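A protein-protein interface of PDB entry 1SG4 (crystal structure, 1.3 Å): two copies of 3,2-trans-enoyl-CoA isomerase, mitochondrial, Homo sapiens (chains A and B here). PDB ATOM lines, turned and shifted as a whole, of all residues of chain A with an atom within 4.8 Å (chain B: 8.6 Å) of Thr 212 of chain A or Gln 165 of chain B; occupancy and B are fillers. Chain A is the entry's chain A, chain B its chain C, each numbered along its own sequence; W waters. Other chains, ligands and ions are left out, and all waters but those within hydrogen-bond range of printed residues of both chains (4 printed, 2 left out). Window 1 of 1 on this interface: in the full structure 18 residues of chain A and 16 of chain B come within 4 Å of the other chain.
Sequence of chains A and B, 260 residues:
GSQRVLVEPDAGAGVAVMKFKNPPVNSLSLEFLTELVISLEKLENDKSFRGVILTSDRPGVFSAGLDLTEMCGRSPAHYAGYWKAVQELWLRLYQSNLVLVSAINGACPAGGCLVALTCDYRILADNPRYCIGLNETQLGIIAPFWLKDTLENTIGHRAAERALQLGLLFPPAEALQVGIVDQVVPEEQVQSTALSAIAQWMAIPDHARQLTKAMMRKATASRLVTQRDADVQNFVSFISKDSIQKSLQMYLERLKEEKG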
ATOM      1  N   ASP A 120       8.312 -20.395 -13.647  1.00  0.00           N
ATOM      2  CA  ASP A 120       7.511 -21.069 -12.652  1.00  0.00           C
ATOM      3  C   ASP A 120       7.290 -22.528 -12.964  1.00  0.00           C
ATOM      4  O   ASP A 120       6.970 -23.337 -12.093  1.00  0.00           O
ATOM      5  CB  ASP A 120       6.167 -20.372 -12.490  1.00  0.00           C
ATOM      6  CG  ASP A 120       6.343 -18.940 -11.978  1.00  0.00           C
ATOM      7  OD1 ASP A 120       7.170 -18.743 -11.045  1.00  0.00           O
ATOM      8  OD2 ASP A 120       5.659 -18.036 -12.506  1.00  0.00           O
ATOM      9  N   TRP A 201      -2.111 -22.114 -13.675  1.00  0.00           N
ATOM     10  CA  TRP A 201      -1.397 -21.149 -12.846  1.00  0.00           C
ATOM     11  C   TRP A 201      -2.073 -19.809 -12.839  1.00  0.00           C
ATOM     12  O   TRP A 201      -2.134 -19.037 -11.877  1.00  0.00           O
ATOM     13  CB  TRP A 201       0.022 -21.007 -13.413  1.00  0.00           C
ATOM     14  CG  TRP A 201       0.923 -22.098 -12.965  1.00  0.00           C
ATOM     15  CD1 TRP A 201       0.970 -23.378 -13.415  1.00  0.00           C
ATOM     16  CD2 TRP A 201       1.897 -22.037 -11.924  1.00  0.00           C
ATOM     17  NE1 TRP A 201       1.917 -24.109 -12.771  1.00  0.00           N
ATOM     18  CE2 TRP A 201       2.507 -23.310 -11.830  1.00  0.00           C
ATOM     19  CE3 TRP A 201       2.321 -21.011 -11.068  1.00  0.00           C
ATOM     20  CZ2 TRP A 201       3.509 -23.601 -10.923  1.00  0.00           C
ATOM     21  CZ3 TRP A 201       3.317 -21.335 -10.183  1.00  0.00           C
ATOM     22  CH2 TRP A 201       3.897 -22.591 -10.107  1.00  0.00           C
ATOM     23  N   ILE A 204      -5.128 -19.046 -10.289  1.00  0.00           N
ATOM     24  CA  ILE A 204      -4.929 -18.732  -8.881  1.00  0.00           C
ATOM     25  C   ILE A 204      -5.187 -17.256  -8.653  1.00  0.00           C
ATOM     26  O   ILE A 204      -4.782 -16.421  -9.485  1.00  0.00           O
ATOM     27  CB  ILE A 204      -3.482 -19.060  -8.433  1.00  0.00           C
ATOM     28  CG1 ILE A 204      -3.082 -20.486  -8.817  1.00  0.00           C
ATOM     29  CG2 ILE A 204      -3.293 -18.775  -6.968  1.00  0.00           C
ATOM     30  CD1 ILE A 204      -3.974 -21.573  -8.260  1.00  0.00           C
ATOM     31  N   ALA A 208      -2.394 -13.182  -4.269  1.00  0.00           N
ATOM     32  CA  ALA A 208      -1.887 -14.223  -3.354  1.00  0.00           C
ATOM     33  C   ALA A 208      -0.799 -15.051  -4.003  1.00  0.00           C
ATOM     34  O   ALA A 208       0.210 -15.401  -3.392  1.00  0.00           O
ATOM     35  CB  ALA A 208      -3.003 -15.147  -2.904  1.00  0.00           C
ATOM     36  N   ARG A 209      -0.989 -15.393  -5.286  1.00  0.00           N
ATOM     37  CA  ARG A 209       0.070 -16.094  -6.004  1.00  0.00           C
ATOM     38  C   ARG A 209       1.361 -15.276  -6.020  1.00  0.00           C
ATOM     39  O   ARG A 209       2.442 -15.795  -5.749  1.00  0.00           O
ATOM     40  CB  ARG A 209      -0.319 -16.382  -7.455  1.00  0.00           C
ATOM     41  CG  ARG A 209       0.739 -17.098  -8.244  1.00  0.00           C
ATOM     42  CD  ARG A 209       0.394 -17.213  -9.727  1.00  0.00           C
ATOM     43  NE  ARG A 209       0.147 -15.899 -10.298  1.00  0.00           N
ATOM     44  CZ  ARG A 209       1.041 -14.995 -10.645  1.00  0.00           C
ATOM     45  NH1 ARG A 209       2.315 -15.224 -10.503  1.00  0.00           N
ATOM     46  NH2 ARG A 209       0.628 -13.832 -11.135  1.00  0.00           N
ATOM     47  N   GLN A 210       1.240 -13.985  -6.366  1.00  0.00           N
ATOM     48  CA  GLN A 210       2.428 -13.131  -6.451  1.00  0.00           C
ATOM     49  C   GLN A 210       3.136 -13.047  -5.111  1.00  0.00           C
ATOM     50  O   GLN A 210       4.365 -13.079  -5.086  1.00  0.00           O
ATOM     51  CB  GLN A 210       2.061 -11.704  -6.916  1.00  0.00           C
ATOM     52  CG  GLN A 210       1.692 -11.679  -8.368  1.00  0.00           C
ATOM     53  CD  GLN A 210       1.050 -10.398  -8.830  1.00  0.00           C
ATOM     54  OE1 GLN A 210       0.500 -10.294  -9.925  1.00  0.00           O
ATOM     55  NE2 GLN A 210       1.162  -9.379  -8.012  1.00  0.00           N
ATOM     56  N   LEU A 211       2.376 -12.866  -4.021  1.00  0.00           N
ATOM     57  CA  LEU A 211       2.997 -12.751  -2.707  1.00  0.00           C
ATOM     58  C   LEU A 211       3.719 -14.035  -2.324  1.00  0.00           C
ATOM     59  O   LEU A 211       4.792 -14.014  -1.710  1.00  0.00           O
ATOM     60  CB  LEU A 211       1.954 -12.401  -1.631  1.00  0.00           C
ATOM     61  CG  LEU A 211       1.433 -10.974  -1.651  1.00  0.00           C
ATOM     62  CD1 LEU A 211       0.248 -10.816  -0.707  1.00  0.00           C
ATOM     63  CD2 LEU A 211       2.556 -10.008  -1.304  1.00  0.00           C
ATOM     64  N   THR A 212       3.103 -15.153  -2.710  1.00  0.00           N
ATOM     65  CA  THR A 212       3.691 -16.442  -2.390  1.00  0.00           C
ATOM     66  C   THR A 212       4.986 -16.659  -3.144  1.00  0.00           C
ATOM     67  O   THR A 212       5.983 -17.083  -2.572  1.00  0.00           O
ATOM     68  CB  THR A 212       2.673 -17.527  -2.731  1.00  0.00           C
ATOM     69  OG1 THR A 212       1.536 -17.367  -1.871  1.00  0.00           O
ATOM     70  CG2 THR A 212       3.246 -18.903  -2.453  1.00  0.00           C
ATOM     71  N   LYS A 213       4.978 -16.347  -4.434  1.00  0.00           N
ATOM     72  CA  LYS A 213       6.168 -16.439  -5.275  1.00  0.00           C
ATOM     73  C   LYS A 213       7.295 -15.593  -4.697  1.00  0.00           C
ATOM     74  O   LYS A 213       8.442 -16.036  -4.570  1.00  0.00           O
ATOM     75  CB  LYS A 213       5.814 -15.976  -6.689  1.00  0.00           C
ATOM     76  CG  LYS A 213       6.978 -16.125  -7.653  1.00  0.00           C
ATOM     77  CD  LYS A 213       6.452 -15.772  -9.049  1.00  0.00           C
ATOM     78  CE  LYS A 213       7.526 -15.798 -10.069  1.00  0.00           C
ATOM     79  NZ  LYS A 213       7.025 -15.715 -11.467  1.00  0.00           N
ATOM     80  N   ALA A 214       6.973 -14.370  -4.316  1.00  0.00           N
ATOM     81  CA  ALA A 214       7.971 -13.447  -3.782  1.00  0.00           C
ATOM     82  C   ALA A 214       8.529 -13.973  -2.494  1.00  0.00           C
ATOM     83  O   ALA A 214       9.745 -13.942  -2.222  1.00  0.00           O
ATOM     84  CB  ALA A 214       7.365 -12.056  -3.635  1.00  0.00           C
ATOM     85  N   MET A 215       7.716 -14.514  -1.619  1.00  0.00           N
ATOM     86  CA  MET A 215       8.242 -15.059  -0.359  1.00  0.00           C
ATOM     87  C   MET A 215       9.211 -16.190  -0.578  1.00  0.00           C
ATOM     88  O   MET A 215      10.183 -16.404   0.159  1.00  0.00           O
ATOM     89  CB  MET A 215       7.021 -15.496   0.468  1.00  0.00           C
ATOM     90  CG  MET A 215       7.344 -16.074   1.832  1.00  0.00           C
ATOM     91  SD  MET A 215       5.892 -16.593   2.738  1.00  0.00           S
ATOM     92  CE  MET A 215       4.904 -17.503   1.551  1.00  0.00           C
ATOM     93  N   MET A 216       9.034 -17.026  -1.595  1.00  0.00           N
ATOM     94  CA  MET A 216       9.830 -18.148  -1.947  1.00  0.00           C
ATOM     95  C   MET A 216      11.186 -17.742  -2.578  1.00  0.00           C
ATOM     96  O   MET A 216      12.153 -18.479  -2.480  1.00  0.00           O
ATOM     97  CB  MET A 216       9.168 -19.052  -2.991  1.00  0.00           C
ATOM     98  CG  MET A 216       7.924 -19.817  -2.648  1.00  0.00           C
ATOM     99  SD  MET A 216       7.996 -20.667  -1.108  1.00  0.00           S
ATOM    100  CE  MET A 216       9.271 -21.928  -1.328  1.00  0.00           C
ATOM    101  N   LEU B 134      -1.398 -27.197   1.355  1.00  0.00           N
ATOM    102  CA  LEU B 134      -1.516 -25.808   1.803  1.00  0.00           C
ATOM    103  C   LEU B 134      -2.181 -25.004   0.704  1.00  0.00           C
ATOM    104  O   LEU B 134      -1.526 -24.500  -0.205  1.00  0.00           O
ATOM    105  CB  LEU B 134      -0.143 -25.277   2.189  1.00  0.00           C
ATOM    106  CG  LEU B 134       0.519 -25.903   3.432  1.00  0.00           C
ATOM    107  CD1 LEU B 134       1.835 -25.199   3.738  1.00  0.00           C
ATOM    108  CD2 LEU B 134      -0.381 -25.848   4.629  1.00  0.00           C
ATOM    109  N   ASN B 135      -3.488 -24.942   0.797  1.00  0.00           N
ATOM    110  CA  ASN B 135      -4.323 -24.372  -0.263  1.00  0.00           C
ATOM    111  C   ASN B 135      -4.769 -22.947   0.002  1.00  0.00           C
ATOM    112  O   ASN B 135      -5.770 -22.469  -0.585  1.00  0.00           O
ATOM    113  CB  ASN B 135      -5.531 -25.288  -0.531  1.00  0.00           C
ATOM    114  CG  ASN B 135      -6.443 -25.428   0.666  1.00  0.00           C
ATOM    115  OD1 ASN B 135      -6.031 -25.315   1.813  1.00  0.00           O
ATOM    116  ND2 ASN B 135      -7.728 -25.653   0.422  1.00  0.00           N
ATOM    117  N   GLU B 136      -4.064 -22.200   0.816  1.00  0.00           N
ATOM    118  CA  GLU B 136      -4.329 -20.802   1.173  1.00  0.00           C
ATOM    119  C   GLU B 136      -4.578 -19.934  -0.043  1.00  0.00           C
ATOM    120  O   GLU B 136      -5.536 -19.106  -0.036  1.00  0.00           O
ATOM    121  CB  GLU B 136      -3.160 -20.229   1.988  1.00  0.00           C
ATOM    122  CG  GLU B 136      -3.078 -20.670   3.434  1.00  0.00           C
ATOM    123  CD  GLU B 136      -2.201 -21.882   3.638  1.00  0.00           C
ATOM    124  OE1 GLU B 136      -2.132 -22.756   2.778  1.00  0.00           O
ATOM    125  OE2 GLU B 136      -1.589 -21.978   4.733  1.00  0.00           O
ATOM    126  N   THR B 137      -3.780 -20.088  -1.107  1.00  0.00           N
ATOM    127  CA  THR B 137      -3.982 -19.159  -2.220  1.00  0.00           C
ATOM    128  C   THR B 137      -5.337 -19.323  -2.870  1.00  0.00           C
ATOM    129  O   THR B 137      -5.795 -18.391  -3.548  1.00  0.00           O
ATOM    130  CB  THR B 137      -2.874 -19.291  -3.293  1.00  0.00           C
ATOM    131  OG1 THR B 137      -2.762 -20.645  -3.730  1.00  0.00           O
ATOM    132  CG2 THR B 137      -1.537 -18.823  -2.734  1.00  0.00           C
ATOM    133  N   GLN B 138      -6.019 -20.465  -2.694  1.00  0.00           N
ATOM    134  CA  GLN B 138      -7.339 -20.594  -3.281  1.00  0.00           C
ATOM    135  C   GLN B 138      -8.336 -19.538  -2.781  1.00  0.00           C
ATOM    136  O   GLN B 138      -9.264 -19.212  -3.513  1.00  0.00           O
ATOM    137  CB  GLN B 138      -7.914 -21.991  -3.001  1.00  0.00           C
ATOM    138  CG  GLN B 138      -7.163 -23.140  -3.634  1.00  0.00           C
ATOM    139  CD  GLN B 138      -7.265 -23.200  -5.125  1.00  0.00           C
ATOM    140  OE1 GLN B 138      -8.221 -22.802  -5.790  1.00  0.00           O
ATOM    141  NE2 GLN B 138      -6.237 -23.786  -5.677  1.00  0.00           N
ATOM    142  N   GLY B 140      -7.255 -16.589  -1.742  1.00  0.00           N
ATOM    143  CA  GLY B 140      -6.608 -15.298  -1.809  1.00  0.00           C
ATOM    144  C   GLY B 140      -5.743 -14.977  -0.603  1.00  0.00           C
ATOM    145  O   GLY B 140      -5.407 -13.795  -0.396  1.00  0.00           O
ATOM    146  N   ILE B 141      -5.385 -15.993   0.157  1.00  0.00           N
ATOM    147  CA  ILE B 141      -4.596 -15.852   1.374  1.00  0.00           C
ATOM    148  C   ILE B 141      -3.263 -16.528   1.115  1.00  0.00           C
ATOM    149  O   ILE B 141      -3.082 -17.229   0.112  1.00  0.00           O
ATOM    150  CB  ILE B 141      -5.291 -16.202   2.696  1.00  0.00           C
ATOM    151  CG1 ILE B 141      -5.907 -17.573   2.820  1.00  0.00           C
ATOM    152  CG2 ILE B 141      -6.373 -15.147   2.983  1.00  0.00           C
ATOM    153  CD1 ILE B 141      -6.440 -17.895   4.205  1.00  0.00           C
ATOM    154  N   ILE B 142      -2.285 -16.301   1.948  1.00  0.00           N
ATOM    155  CA  ILE B 142      -0.994 -16.942   1.769  1.00  0.00           C
ATOM    156  C   ILE B 142      -0.608 -17.664   3.045  1.00  0.00           C
ATOM    157  O   ILE B 142      -1.075 -17.324   4.120  1.00  0.00           O
ATOM    158  CB  ILE B 142       0.092 -15.935   1.359  1.00  0.00           C
ATOM    159  CG1 ILE B 142       0.456 -14.863   2.379  1.00  0.00           C
ATOM    160  CG2 ILE B 142      -0.315 -15.253   0.053  1.00  0.00           C
ATOM    161  CD1 ILE B 142       1.821 -14.314   1.982  1.00  0.00           C
ATOM    162  N   ALA B 143       0.226 -18.688   2.907  1.00  0.00           N
ATOM    163  CA  ALA B 143       0.784 -19.296   4.110  1.00  0.00           C
ATOM    164  C   ALA B 143       1.770 -18.368   4.786  1.00  0.00           C
ATOM    165  O   ALA B 143       2.541 -17.662   4.128  1.00  0.00           O
ATOM    166  CB  ALA B 143       1.447 -20.614   3.756  1.00  0.00           C
ATOM    167  N   PRO B 144       1.795 -18.355   6.111  1.00  0.00           N
ATOM    168  CA  PRO B 144       2.783 -17.527   6.810  1.00  0.00           C
ATOM    169  C   PRO B 144       4.174 -18.111   6.547  1.00  0.00           C
ATOM    170  O   PRO B 144       4.315 -19.289   6.219  1.00  0.00           O
ATOM    171  CB  PRO B 144       2.416 -17.666   8.273  1.00  0.00           C
ATOM    172  CG  PRO B 144       1.585 -18.888   8.363  1.00  0.00           C
ATOM    173  CD  PRO B 144       0.902 -19.098   7.022  1.00  0.00           C
ATOM    174  N   LYS B 148       5.336 -21.953   5.397  1.00  0.00           N
ATOM    175  CA  LYS B 148       6.090 -22.181   4.168  1.00  0.00           C
ATOM    176  C   LYS B 148       7.410 -22.884   4.502  1.00  0.00           C
ATOM    177  O   LYS B 148       7.785 -23.824   3.808  1.00  0.00           O
ATOM    178  CB  LYS B 148       6.323 -20.832   3.483  1.00  0.00           C
ATOM    179  CG  LYS B 148       7.239 -20.885   2.263  1.00  0.00           C
ATOM    180  CD  LYS B 148       8.724 -20.697   2.509  1.00  0.00           C
ATOM    181  CE  LYS B 148       9.040 -19.301   2.939  1.00  0.00           C
ATOM    182  NZ  LYS B 148      10.515 -19.146   3.194  1.00  0.00           N
ATOM    183  N   LEU B 151       6.790 -26.457   5.203  1.00  0.00           N
ATOM    184  CA  LEU B 151       6.564 -27.203   3.957  1.00  0.00           C
ATOM    185  C   LEU B 151       7.861 -27.443   3.188  1.00  0.00           C
ATOM    186  O   LEU B 151       8.074 -28.571   2.723  1.00  0.00           O
ATOM    187  CB  LEU B 151       5.518 -26.497   3.091  1.00  0.00           C
ATOM    188  CG  LEU B 151       5.138 -27.302   1.826  1.00  0.00           C
ATOM    189  CD1 LEU B 151       4.435 -28.613   2.169  1.00  0.00           C
ATOM    190  CD2 LEU B 151       4.321 -26.462   0.891  1.00  0.00           C
ATOM    191  N   HIS B 157      12.450 -27.154  -1.777  1.00  0.00           N
ATOM    192  CA  HIS B 157      12.092 -25.845  -2.288  1.00  0.00           C
ATOM    193  C   HIS B 157      11.209 -25.888  -3.534  1.00  0.00           C
ATOM    194  O   HIS B 157      10.201 -25.159  -3.591  1.00  0.00           O
ATOM    195  CB  HIS B 157      13.374 -25.032  -2.577  1.00  0.00           C
ATOM    196  CG  HIS B 157      13.074 -23.630  -2.989  1.00  0.00           C
ATOM    197  ND1 HIS B 157      13.089 -22.594  -2.080  1.00  0.00           N
ATOM    198  CD2 HIS B 157      12.727 -23.066  -4.186  1.00  0.00           C
ATOM    199  CE1 HIS B 157      12.765 -21.446  -2.693  1.00  0.00           C
ATOM    200  NE2 HIS B 157      12.538 -21.699  -3.965  1.00  0.00           N
ATOM    201  N   ARG B 158      11.599 -26.648  -4.550  1.00  0.00           N
ATOM    202  CA  ARG B 158      10.883 -26.550  -5.835  1.00  0.00           C
ATOM    203  C   ARG B 158       9.420 -26.954  -5.618  1.00  0.00           C
ATOM    204  O   ARG B 158       8.483 -26.316  -6.102  1.00  0.00           O
ATOM    205  CB  ARG B 158      11.593 -27.394  -6.882  1.00  0.00           C
ATOM    206  CG  ARG B 158      11.121 -27.138  -8.297  1.00  0.00           C
ATOM    207  CD  ARG B 158       9.866 -27.916  -8.694  1.00  0.00           C
ATOM    208  NE  ARG B 158       9.233 -27.332  -9.900  1.00  0.00           N
ATOM    209  CZ  ARG B 158       8.540 -26.225  -9.987  1.00  0.00           C
ATOM    210  NH1 ARG B 158       8.329 -25.492  -8.894  1.00  0.00           N
ATOM    211  NH2 ARG B 158       8.038 -25.819 -11.145  1.00  0.00           N
ATOM    212  N   ALA B 159       9.258 -28.092  -4.940  1.00  0.00           N
ATOM    213  CA  ALA B 159       7.899 -28.610  -4.756  1.00  0.00           C
ATOM    214  C   ALA B 159       7.083 -27.672  -3.915  1.00  0.00           C
ATOM    215  O   ALA B 159       5.875 -27.461  -4.180  1.00  0.00           O
ATOM    216  CB  ALA B 159       7.958 -30.027  -4.193  1.00  0.00           C
ATOM    217  N   ALA B 160       7.679 -27.062  -2.895  1.00  0.00           N
ATOM    218  CA  ALA B 160       6.927 -26.086  -2.117  1.00  0.00           C
ATOM    219  C   ALA B 160       6.538 -24.838  -2.917  1.00  0.00           C
ATOM    220  O   ALA B 160       5.467 -24.326  -2.722  1.00  0.00           O
ATOM    221  CB  ALA B 160       7.777 -25.718  -0.914  1.00  0.00           C
ATOM    222  N   GLU B 161       7.443 -24.405  -3.812  1.00  0.00           N
ATOM    223  CA  GLU B 161       7.149 -23.239  -4.608  1.00  0.00           C
ATOM    224  C   GLU B 161       5.853 -23.481  -5.402  1.00  0.00           C
ATOM    225  O   GLU B 161       4.942 -22.655  -5.483  1.00  0.00           O
ATOM    226  CB  GLU B 161       8.296 -22.939  -5.535  1.00  0.00           C
ATOM    227  CG  GLU B 161       8.605 -21.596  -5.975  1.00  0.00           C
ATOM    228  CD  GLU B 161       9.886 -21.429  -6.754  1.00  0.00           C
ATOM    229  OE1 GLU B 161       9.809 -21.805  -7.928  1.00  0.00           O
ATOM    230  OE2 GLU B 161      10.920 -20.978  -6.216  1.00  0.00           O
ATOM    231  N   ARG B 162       5.776 -24.631  -6.051  1.00  0.00           N
ATOM    232  CA  ARG B 162       4.611 -24.999  -6.840  1.00  0.00           C
ATOM    233  C   ARG B 162       3.349 -25.247  -6.000  1.00  0.00           C
ATOM    234  O   ARG B 162       2.277 -24.742  -6.273  1.00  0.00           O
ATOM    235  CB  ARG B 162       4.920 -26.234  -7.738  1.00  0.00           C
ATOM    236  CG  ARG B 162       3.679 -26.768  -8.427  1.00  0.00           C
ATOM    237  CD  ARG B 162       4.085 -27.812  -9.455  1.00  0.00           C
ATOM    238  NE  ARG B 162       2.923 -28.477 -10.039  1.00  0.00           N
ATOM    239  CZ  ARG B 162       2.315 -29.549  -9.546  1.00  0.00           C
ATOM    240  NH1 ARG B 162       2.740 -30.137  -8.448  1.00  0.00           N
ATOM    241  NH2 ARG B 162       1.270 -30.018 -10.211  1.00  0.00           N
ATOM    242  N   ALA B 163       3.516 -26.027  -4.936  1.00  0.00           N
ATOM    243  CA  ALA B 163       2.395 -26.416  -4.091  1.00  0.00           C
ATOM    244  C   ALA B 163       1.748 -25.207  -3.448  1.00  0.00           C
ATOM    245  O   ALA B 163       0.518 -25.101  -3.368  1.00  0.00           O
ATOM    246  CB  ALA B 163       2.837 -27.413  -3.048  1.00  0.00           C
ATOM    247  N   LEU B 164       2.565 -24.276  -2.993  1.00  0.00           N
ATOM    248  CA  LEU B 164       2.022 -23.087  -2.348  1.00  0.00           C
ATOM    249  C   LEU B 164       1.408 -22.138  -3.346  1.00  0.00           C
ATOM    250  O   LEU B 164       0.320 -21.621  -3.108  1.00  0.00           O
ATOM    251  CB  LEU B 164       3.105 -22.375  -1.546  1.00  0.00           C
ATOM    252  CG  LEU B 164       3.484 -23.064  -0.264  1.00  0.00           C
ATOM    253  CD1 LEU B 164       4.801 -22.584   0.279  1.00  0.00           C
ATOM    254  CD2 LEU B 164       2.326 -22.843   0.730  1.00  0.00           C
ATOM    255  N   GLN B 165       2.076 -21.884  -4.458  1.00  0.00           N
ATOM    256  CA  GLN B 165       1.460 -20.959  -5.444  1.00  0.00           C
ATOM    257  C   GLN B 165       0.143 -21.465  -5.981  1.00  0.00           C
ATOM    258  O   GLN B 165      -0.827 -20.705  -6.048  1.00  0.00           O
ATOM    259  CB  GLN B 165       2.416 -20.668  -6.575  1.00  0.00           C
ATOM    260  CG  GLN B 165       3.485 -19.672  -6.121  1.00  0.00           C
ATOM    261  CD  GLN B 165       4.437 -19.392  -7.251  1.00  0.00           C
ATOM    262  OE1 GLN B 165       4.141 -18.572  -8.098  1.00  0.00           O
ATOM    263  NE2 GLN B 165       5.585 -20.053  -7.225  1.00  0.00           N
ATOM    264  N   LEU B 166       0.094 -22.738  -6.355  1.00  0.00           N
ATOM    265  CA  LEU B 166      -1.116 -23.341  -6.890  1.00  0.00           C
ATOM    266  C   LEU B 166      -2.101 -23.721  -5.810  1.00  0.00           C
ATOM    267  O   LEU B 166      -3.232 -24.108  -6.127  1.00  0.00           O
ATOM    268  CB  LEU B 166      -0.752 -24.572  -7.700  1.00  0.00           C
ATOM    269  CG  LEU B 166      -0.056 -24.330  -9.008  1.00  0.00           C
ATOM    270  CD1 LEU B 166       0.280 -25.641  -9.701  1.00  0.00           C
ATOM    271  CD2 LEU B 166      -0.869 -23.489  -9.976  1.00  0.00           C
ATOM    272  N   GLY B 167      -1.709 -23.618  -4.547  1.00  0.00           N
ATOM    273  CA  GLY B 167      -2.630 -23.946  -3.474  1.00  0.00           C
ATOM    274  C   GLY B 167      -3.147 -25.365  -3.597  1.00  0.00           C
ATOM    275  O   GLY B 167      -4.340 -25.590  -3.489  1.00  0.00           O
ATOM    276  N   LEU B 168      -2.253 -26.315  -3.864  1.00  0.00           N
ATOM    277  CA  LEU B 168      -2.619 -27.680  -4.195  1.00  0.00           C
ATOM    278  C   LEU B 168      -2.993 -28.522  -3.003  1.00  0.00           C
ATOM    279  O   LEU B 168      -2.381 -28.437  -1.967  1.00  0.00           O
ATOM    280  CB  LEU B 168      -1.449 -28.396  -4.881  1.00  0.00           C
ATOM    281  CG  LEU B 168      -0.965 -27.907  -6.209  1.00  0.00           C
ATOM    282  CD1 LEU B 168       0.182 -28.790  -6.673  1.00  0.00           C
ATOM    283  CD2 LEU B 168      -2.139 -27.903  -7.230  1.00  0.00           C
ATOM    284  N   PHE B 238      -2.888  -8.018   7.076  1.00  0.00           N
ATOM    285  CA  PHE B 238      -3.281  -8.738   5.870  1.00  0.00           C
ATOM    286  C   PHE B 238      -4.734  -9.174   5.928  1.00  0.00           C
ATOM    287  O   PHE B 238      -5.492  -8.890   4.988  1.00  0.00           O
ATOM    288  CB  PHE B 238      -2.319  -9.914   5.697  1.00  0.00           C
ATOM    289  CG  PHE B 238      -2.599 -10.762   4.478  1.00  0.00           C
ATOM    290  CD1 PHE B 238      -3.363 -11.895   4.576  1.00  0.00           C
ATOM    291  CD2 PHE B 238      -2.091 -10.399   3.237  1.00  0.00           C
ATOM    292  CE1 PHE B 238      -3.655 -12.639   3.467  1.00  0.00           C
ATOM    293  CE2 PHE B 238      -2.383 -11.142   2.102  1.00  0.00           C
ATOM    294  CZ  PHE B 238      -3.157 -12.278   2.230  1.00  0.00           C
HETATM  295  O   HOH W   1       7.144 -22.946  -9.334  1.00  0.00           O
HETATM  296  O   HOH W   2       7.600 -20.347  -9.088  1.00  0.00           O
HETATM  297  O   HOH W   3       3.633 -17.651 -10.579  1.00  0.00           O
HETATM  298  O   HOH W   4       0.803 -19.443   0.177  1.00  0.00           O
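No position is printed for both chains.
Of the 23 pairs that touch across the chains among the printed residues, none has its exchanged pair printed and touching as well.
Of the 12 printed residues of chain A, 10 touch a printed residue of chain B.
Among the printed residues, 23 pairs touch across the chains.
Among the printed residues, no Asp or Glu carboxylate lies within 4 Å of a Lys or Arg side-chain nitrogen of the other chain.
Water W2 lies within hydrogen-bond range of the side-chain carboxylate (OD1) of Asp 120 of chain A (2.6 Å), the side-chain amide nitrogen (NE2) of Gln 165 of chain B (2.8 Å) and the side-chain carboxylate (OE1) of Glu 161 of chain B (2.9 Å).
Thr 212 of chain A touches just these residues of chain B: Thr 137 (3.5 Å), Ile 142 (3.4 Å), Leu 164 (3.6 Å) and Gln 165 (3.8 Å).
Gln 138 of chain B touches none of the printed residues of chain A.
Of the printed residues of chain A, Gly 140 of chain B touches Ala 208.
Printed residues of chain A within 4 Å of Lys 148 of chain B: Met 215 and Met 216.
Leu 151 of chain B touches none of the printed residues of chain A.
Of chain A, only Trp 201, Ile 204, Arg 209, Thr 212 and Lys 213 come within 4 Å of Gln 165 of chain B.
The nearest printed residue of chain B that does not touch Thr 212 of chain A is Ile 141 of chain B (5.0 Å).
The nearest residue of chain A that does not touch Gln 165 of chain B is Asp 120 of chain A (4.2 Å).
The nearest printed residue of chain A that does not touch Leu 166 of chain B is Arg 209 of chain A (6.0 Å).
O of Glu 136 of chain B lies within hydrogen-bond range of N of Ile 141 of chain B, 3.1 Å away.
OG1 of Thr 137 of chain B is in hydrogen-bond range of O of Gln 165 of chain B (3.0 Å).
NE2 of Gln 138 of chain B sits at hydrogen-bond distance from O of Leu 166 of chain B.
O of Glu 161 of chain B sits at hydrogen-bond distance from NE2 of Gln 165 of chain B, at 3.2 Å.
Among the printed residues, pairs that only touch across the chains: Met 216 of chain A with His 157 of chain B (3.0 Å), Ile 204 of chain A with Gln 165 of chain B (3.3 Å), Lys 213 of chain A with Gln 165 of chain B (3.4 Å), Ile 204 of chain A with Leu 166 of chain B (3.4 Å), Thr 212 of chain A with Ile 142 of chain B (3.4 Å), Met 216 of chain A with Lys 148 of chain B (3.5 Å), Ala 208 of chain A with Ile 142 of chain B (3.5 Å), Thr 212 of chain A with Thr 137 of chain B (3.5 Å), Trp 201 of chain A with Gln 165 of chain B (3.6 Å), Ala 208 of chain A with Gly 140 of chain B (3.6 Å), Thr 212 of chain A with Leu 164 of chain B (3.6 Å), Ala 208 of chain A with Ile 141 of chain B (3.7 Å), Trp 201 of chain A with Leu 166 of chain B (3.7 Å), Arg 209 of chain A with Gln 165 of chain B (3.7 Å), Ile 204 of chain A with Thr 137 of chain B (3.7 Å), Thr 212 of chain A with Gln 165 of chain B (3.8 Å), Met 215 of chain A with Lys 148 of chain B (3.8 Å), Met 216 of chain A with Glu 161 of chain B (3.8 Å), Leu 211 of chain A with Phe 238 of chain B (3.9 Å), Ala 208 of chain A with Thr 137 of chain B (3.9 Å) and Met 216 of chain A with Leu 164 of chain B (3.98 Å).
The guanidinium group of Arg 158 of chain B lies within hydrogen-bond range of the backbone carbonyl oxygen of Asp 120 of chain A (2.9 Å).
SD of Met 215 of chain A sits close to O of Ala 143 of chain B.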
